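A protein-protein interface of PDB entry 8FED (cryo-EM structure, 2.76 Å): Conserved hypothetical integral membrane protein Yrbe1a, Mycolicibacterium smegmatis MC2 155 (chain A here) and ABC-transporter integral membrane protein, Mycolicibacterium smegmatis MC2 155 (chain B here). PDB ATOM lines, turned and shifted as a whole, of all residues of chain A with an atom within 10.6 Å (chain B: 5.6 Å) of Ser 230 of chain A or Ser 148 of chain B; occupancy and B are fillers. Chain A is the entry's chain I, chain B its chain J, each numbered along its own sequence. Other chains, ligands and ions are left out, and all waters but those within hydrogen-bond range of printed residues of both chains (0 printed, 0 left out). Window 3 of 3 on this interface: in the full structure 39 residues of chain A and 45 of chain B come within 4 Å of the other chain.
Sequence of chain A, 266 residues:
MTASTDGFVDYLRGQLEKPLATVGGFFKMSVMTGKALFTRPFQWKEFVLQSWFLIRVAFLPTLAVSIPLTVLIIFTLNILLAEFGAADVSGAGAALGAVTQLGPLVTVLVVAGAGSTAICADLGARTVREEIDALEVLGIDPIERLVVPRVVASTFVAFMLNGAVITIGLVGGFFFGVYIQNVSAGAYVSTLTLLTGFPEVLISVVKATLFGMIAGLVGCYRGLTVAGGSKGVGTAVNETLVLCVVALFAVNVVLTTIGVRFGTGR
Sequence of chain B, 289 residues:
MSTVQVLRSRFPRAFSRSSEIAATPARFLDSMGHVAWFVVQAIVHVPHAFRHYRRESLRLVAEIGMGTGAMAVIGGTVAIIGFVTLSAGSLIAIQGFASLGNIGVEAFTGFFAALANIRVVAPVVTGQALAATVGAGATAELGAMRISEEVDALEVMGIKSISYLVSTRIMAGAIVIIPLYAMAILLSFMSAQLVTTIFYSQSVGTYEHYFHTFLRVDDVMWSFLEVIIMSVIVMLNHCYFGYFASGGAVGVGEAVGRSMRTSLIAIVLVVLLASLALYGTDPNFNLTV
OG of Ser 148 of chain B sits at hydrogen-bond distance from OG of Ser 230 of chain A, at 3.1 Å.
O of Lys 231 of chain A lies within hydrogen-bond range of OG1 of Thr 235 of chain A, at 2.8 Å. The backbone carbonyl oxygen (O) of Ala 144 of chain B lies within hydrogen-bond range of the side-chain hydroxyl (OG) of Ser 148 of chain B (3.0 Å).
Among the printed residues, pairs that only touch across the chains: Ser 230 of chain A with Ile 147 of chain B (3.9 Å), Lys 231 of chain A with Ala 144 of chain B (3.7 Å), Val 233 of chain A with Ala 249 of chain B (3.3 Å) and Gly 234 of chain A with Val 252 of chain B (3.8 Å).
Ser 230 of chain A touches just these residues of chain B: Ile 147 (3.9 Å) and Ser 148 (3.1 Å). Printed residues of chain B within 4 Å of Lys 231 of chain A: Ala 144 (3.7 Å). Printed residues of chain B within 4 Å of Val 233 of chain A: Ala 249 (3.3 Å). Printed residues of chain B within 4 Å of Gly 234 of chain A: Val 252 (3.8 Å). Gly 143 of chain B touches none of the printed residues of chain A. Of chain A, only Ser 230 (3.9 Å) comes within 4 Å of Ile 147 of chain B. Printed residues of chain A within 4 Å of Ser 148 of chain B: Ser 230 (3.1 Å). No residue of chain A comes within 4 Å of Glu 149 of chain B. No residue of chain A comes within 4 Å of Glu 150 of chain B. Of chain A, only Val 233 (3.3 Å) comes within 4 Å of Ala 249 of chain B. Of the printed residues of chain A, Val 252 of chain B touches Gly 234. The nearest residue of chain A that does not touch Ser 148 of chain B is Lys 231 of chain A (6.4 Å). The nearest printed residue of chain B that does not touch Lys 231 of chain A is Ala 249 of chain B (5.2 Å).
Hydrophobic or aromatic side chains of chain B that line the printed part of chain A: Ala 144, Ile 147 and Val 252. Hydrophobic or aromatic side chains of chain A that line the printed part of chain B: Val 233. Among the printed residues, 5 pairs touch across the chains.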
ATOM      1  N   VAL A 128      25.722 -23.964   0.722  1.00  0.00           N
ATOM      2  CA  VAL A 128      26.221 -23.227  -0.436  1.00  0.00           C
ATOM      3  C   VAL A 128      27.699 -22.886  -0.302  1.00  0.00           C
ATOM      4  O   VAL A 128      28.371 -22.664  -1.316  1.00  0.00           O
ATOM      5  CB  VAL A 128      25.398 -21.947  -0.683  1.00  0.00           C
ATOM      6  CG1 VAL A 128      23.940 -22.287  -0.936  1.00  0.00           C
ATOM      7  CG2 VAL A 128      25.536 -20.976   0.479  1.00  0.00           C
ATOM      8  N   VAL A 226      19.232 -27.159   0.078  1.00  0.00           N
ATOM      9  CA  VAL A 226      19.089 -25.892  -0.625  1.00  0.00           C
ATOM     10  C   VAL A 226      19.599 -26.042  -2.057  1.00  0.00           C
ATOM     11  O   VAL A 226      20.424 -26.913  -2.364  1.00  0.00           O
ATOM     12  CB  VAL A 226      19.827 -24.770   0.129  1.00  0.00           C
ATOM     13  CG1 VAL A 226      21.319 -24.813  -0.151  1.00  0.00           C
ATOM     14  CG2 VAL A 226      19.244 -23.411  -0.218  1.00  0.00           C
ATOM     15  N   ALA A 227      19.079 -25.202  -2.951  1.00  0.00           N
ATOM     16  CA  ALA A 227      19.369 -25.290  -4.377  1.00  0.00           C
ATOM     17  C   ALA A 227      20.458 -24.329  -4.831  1.00  0.00           C
ATOM     18  O   ALA A 227      20.752 -24.275  -6.030  1.00  0.00           O
ATOM     19  CB  ALA A 227      18.095 -25.043  -5.189  1.00  0.00           C
ATOM     20  N   GLY A 228      21.064 -23.584  -3.914  1.00  0.00           N
ATOM     21  CA  GLY A 228      22.111 -22.647  -4.297  1.00  0.00           C
ATOM     22  C   GLY A 228      21.560 -21.520  -5.148  1.00  0.00           C
ATOM     23  O   GLY A 228      20.582 -20.863  -4.780  1.00  0.00           O
ATOM     24  N   GLY A 229      22.191 -21.286  -6.296  1.00  0.00           N
ATOM     25  CA  GLY A 229      21.758 -20.235  -7.197  1.00  0.00           C
ATOM     26  C   GLY A 229      21.853 -18.865  -6.552  1.00  0.00           C
ATOM     27  O   GLY A 229      22.715 -18.598  -5.707  1.00  0.00           O
ATOM     28  N   SER A 230      20.947 -17.975  -6.959  1.00  0.00           N
ATOM     29  CA  SER A 230      20.844 -16.650  -6.366  1.00  0.00           C
ATOM     30  C   SER A 230      19.551 -16.433  -5.596  1.00  0.00           C
ATOM     31  O   SER A 230      19.434 -15.429  -4.886  1.00  0.00           O
ATOM     32  CB  SER A 230      20.972 -15.568  -7.448  1.00  0.00           C
ATOM     33  OG  SER A 230      20.834 -14.274  -6.887  1.00  0.00           O
ATOM     34  N   LYS A 231      18.579 -17.340  -5.719  1.00  0.00           N
ATOM     35  CA  LYS A 231      17.335 -17.265  -4.965  1.00  0.00           C
ATOM     36  C   LYS A 231      17.019 -18.581  -4.261  1.00  0.00           C
ATOM     37  O   LYS A 231      15.935 -18.720  -3.683  1.00  0.00           O
ATOM     38  CB  LYS A 231      16.178 -16.866  -5.894  1.00  0.00           C
ATOM     39  CG  LYS A 231      14.964 -16.253  -5.206  1.00  0.00           C
ATOM     40  CD  LYS A 231      13.764 -16.238  -6.135  1.00  0.00           C
ATOM     41  CE  LYS A 231      12.494 -15.871  -5.391  1.00  0.00           C
ATOM     42  NZ  LYS A 231      11.292 -16.031  -6.253  1.00  0.00           N
ATOM     43  N   GLY A 232      17.938 -19.548  -4.290  1.00  0.00           N
ATOM     44  CA  GLY A 232      17.656 -20.842  -3.689  1.00  0.00           C
ATOM     45  C   GLY A 232      17.476 -20.776  -2.185  1.00  0.00           C
ATOM     46  O   GLY A 232      16.621 -21.467  -1.626  1.00  0.00           O
ATOM     47  N   VAL A 233      18.280 -19.955  -1.508  1.00  0.00           N
ATOM     48  CA  VAL A 233      18.171 -19.840  -0.057  1.00  0.00           C
ATOM     49  C   VAL A 233      16.849 -19.188   0.332  1.00  0.00           C
ATOM     50  O   VAL A 233      16.151 -19.659   1.236  1.00  0.00           O
ATOM     51  CB  VAL A 233      19.375 -19.070   0.514  1.00  0.00           C
ATOM     52  CG1 VAL A 233      19.263 -18.950   2.023  1.00  0.00           C
ATOM     53  CG2 VAL A 233      20.671 -19.759   0.131  1.00  0.00           C
ATOM     54  N   GLY A 234      16.484 -18.098  -0.347  1.00  0.00           N
ATOM     55  CA  GLY A 234      15.223 -17.438  -0.045  1.00  0.00           C
ATOM     56  C   GLY A 234      14.019 -18.306  -0.357  1.00  0.00           C
ATOM     57  O   GLY A 234      13.054 -18.348   0.412  1.00  0.00           O
ATOM     58  N   THR A 235      14.061 -19.011  -1.491  1.00  0.00           N
ATOM     59  CA  THR A 235      12.987 -19.938  -1.828  1.00  0.00           C
ATOM     60  C   THR A 235      12.890 -21.055  -0.798  1.00  0.00           C
ATOM     61  O   THR A 235      11.786 -21.446  -0.400  1.00  0.00           O
ATOM     62  CB  THR A 235      13.216 -20.519  -3.224  1.00  0.00           C
ATOM     63  OG1 THR A 235      13.289 -19.453  -4.179  1.00  0.00           O
ATOM     64  CG2 THR A 235      12.082 -21.454  -3.610  1.00  0.00           C
ATOM     65  N   ALA A 236      14.035 -21.574  -0.351  1.00  0.00           N
ATOM     66  CA  ALA A 236      14.034 -22.625   0.659  1.00  0.00           C
ATOM     67  C   ALA A 236      13.445 -22.130   1.972  1.00  0.00           C
ATOM     68  O   ALA A 236      12.683 -22.849   2.625  1.00  0.00           O
ATOM     69  CB  ALA A 236      15.451 -23.152   0.871  1.00  0.00           C
ATOM     70  N   GLY B 143      14.902  -9.533  -2.868  1.00  0.00           N
ATOM     71  CA  GLY B 143      16.279  -9.822  -2.506  1.00  0.00           C
ATOM     72  C   GLY B 143      17.068 -10.413  -3.656  1.00  0.00           C
ATOM     73  O   GLY B 143      18.231 -10.057  -3.868  1.00  0.00           O
ATOM     74  N   ALA B 144      16.451 -11.321  -4.416  1.00  0.00           N
ATOM     75  CA  ALA B 144      17.113 -11.875  -5.591  1.00  0.00           C
ATOM     76  C   ALA B 144      17.392 -10.794  -6.625  1.00  0.00           C
ATOM     77  O   ALA B 144      18.456 -10.787  -7.254  1.00  0.00           O
ATOM     78  CB  ALA B 144      16.264 -12.989  -6.198  1.00  0.00           C
ATOM     79  N   MET B 145      16.441  -9.878  -6.825  1.00  0.00           N
ATOM     80  CA  MET B 145      16.662  -8.778  -7.759  1.00  0.00           C
ATOM     81  C   MET B 145      17.788  -7.865  -7.288  1.00  0.00           C
ATOM     82  O   MET B 145      18.605  -7.411  -8.096  1.00  0.00           O
ATOM     83  CB  MET B 145      15.372  -7.982  -7.954  1.00  0.00           C
ATOM     84  CG  MET B 145      14.279  -8.749  -8.673  1.00  0.00           C
ATOM     85  SD  MET B 145      12.784  -7.774  -8.909  1.00  0.00           S
ATOM     86  CE  MET B 145      11.715  -8.987  -9.679  1.00  0.00           C
ATOM     87  N   ARG B 146      17.837  -7.572  -5.986  1.00  0.00           N
ATOM     88  CA  ARG B 146      18.901  -6.724  -5.455  1.00  0.00           C
ATOM     89  C   ARG B 146      20.268  -7.383  -5.591  1.00  0.00           C
ATOM     90  O   ARG B 146      21.243  -6.724  -5.972  1.00  0.00           O
ATOM     91  CB  ARG B 146      18.612  -6.383  -3.995  1.00  0.00           C
ATOM     92  CG  ARG B 146      19.736  -5.647  -3.292  1.00  0.00           C
ATOM     93  CD  ARG B 146      19.970  -4.276  -3.895  1.00  0.00           C
ATOM     94  NE  ARG B 146      18.850  -3.374  -3.661  1.00  0.00           N
ATOM     95  CZ  ARG B 146      18.798  -2.122  -4.093  1.00  0.00           C
ATOM     96  NH1 ARG B 146      19.784  -1.592  -4.796  1.00  0.00           N
ATOM     97  NH2 ARG B 146      17.729  -1.384  -3.812  1.00  0.00           N
ATOM     98  N   ILE B 147      20.362  -8.679  -5.286  1.00  0.00           N
ATOM     99  CA  ILE B 147      21.648  -9.365  -5.356  1.00  0.00           C
ATOM    100  C   ILE B 147      22.103  -9.513  -6.803  1.00  0.00           C
ATOM    101  O   ILE B 147      23.275  -9.290  -7.126  1.00  0.00           O
ATOM    102  CB  ILE B 147      21.564 -10.726  -4.642  1.00  0.00           C
ATOM    103  CG1 ILE B 147      21.329 -10.524  -3.145  1.00  0.00           C
ATOM    104  CG2 ILE B 147      22.826 -11.537  -4.874  1.00  0.00           C
ATOM    105  CD1 ILE B 147      22.305  -9.574  -2.496  1.00  0.00           C
ATOM    106  N   SER B 148      21.186  -9.875  -7.698  1.00  0.00           N
ATOM    107  CA  SER B 148      21.495 -10.052  -9.112  1.00  0.00           C
ATOM    108  C   SER B 148      21.652  -8.735  -9.862  1.00  0.00           C
ATOM    109  O   SER B 148      21.700  -8.756 -11.097  1.00  0.00           O
ATOM    110  CB  SER B 148      20.417 -10.901  -9.786  1.00  0.00           C
ATOM    111  OG  SER B 148      20.282 -12.155  -9.142  1.00  0.00           O
ATOM    112  N   GLU B 149      21.704  -7.605  -9.153  1.00  0.00           N
ATOM    113  CA  GLU B 149      21.931  -6.282  -9.732  1.00  0.00           C
ATOM    114  C   GLU B 149      20.821  -5.867 -10.692  1.00  0.00           C
ATOM    115  O   GLU B 149      21.037  -5.024 -11.567  1.00  0.00           O
ATOM    116  CB  GLU B 149      23.296  -6.203 -10.426  1.00  0.00           C
ATOM    117  CG  GLU B 149      24.471  -6.463  -9.499  1.00  0.00           C
ATOM    118  CD  GLU B 149      25.734  -6.838 -10.246  1.00  0.00           C
ATOM    119  OE1 GLU B 149      25.629  -7.282 -11.409  1.00  0.00           O
ATOM    120  OE2 GLU B 149      26.833  -6.690  -9.672  1.00  0.00           O
ATOM    121  N   GLU B 150      19.626  -6.445 -10.543  1.00  0.00           N
ATOM    122  CA  GLU B 150      18.506  -6.050 -11.390  1.00  0.00           C
ATOM    123  C   GLU B 150      17.944  -4.696 -10.984  1.00  0.00           C
ATOM    124  O   GLU B 150      17.467  -3.945 -11.842  1.00  0.00           O
ATOM    125  CB  GLU B 150      17.414  -7.115 -11.345  1.00  0.00           C
ATOM    126  CG  GLU B 150      17.864  -8.472 -11.852  1.00  0.00           C
ATOM    127  CD  GLU B 150      16.732  -9.477 -11.907  1.00  0.00           C
ATOM    128  OE1 GLU B 150      15.560  -9.056 -11.848  1.00  0.00           O
ATOM    129  OE2 GLU B 150      17.016 -10.688 -12.004  1.00  0.00           O
ATOM    130  N   ALA B 249      23.177 -14.412  -1.462  1.00  0.00           N
ATOM    131  CA  ALA B 249      22.017 -15.280  -1.298  1.00  0.00           C
ATOM    132  C   ALA B 249      21.747 -15.625   0.161  1.00  0.00           C
ATOM    133  O   ALA B 249      20.613 -15.981   0.500  1.00  0.00           O
ATOM    134  CB  ALA B 249      22.199 -16.563  -2.109  1.00  0.00           C
ATOM    135  N   VAL B 252      19.250 -13.179   2.122  1.00  0.00           N
ATOM    136  CA  VAL B 252      17.839 -13.225   1.750  1.00  0.00           C
ATOM    137  C   VAL B 252      17.030 -13.971   2.805  1.00  0.00           C
ATOM    138  O   VAL B 252      15.933 -13.541   3.181  1.00  0.00           O
ATOM    139  CB  VAL B 252      17.678 -13.857   0.355  1.00  0.00           C
ATOM    140  CG1 VAL B 252      16.227 -13.811  -0.086  1.00  0.00           C
ATOM    141  CG2 VAL B 252      18.567 -13.145  -0.650  1.00  0.00           C
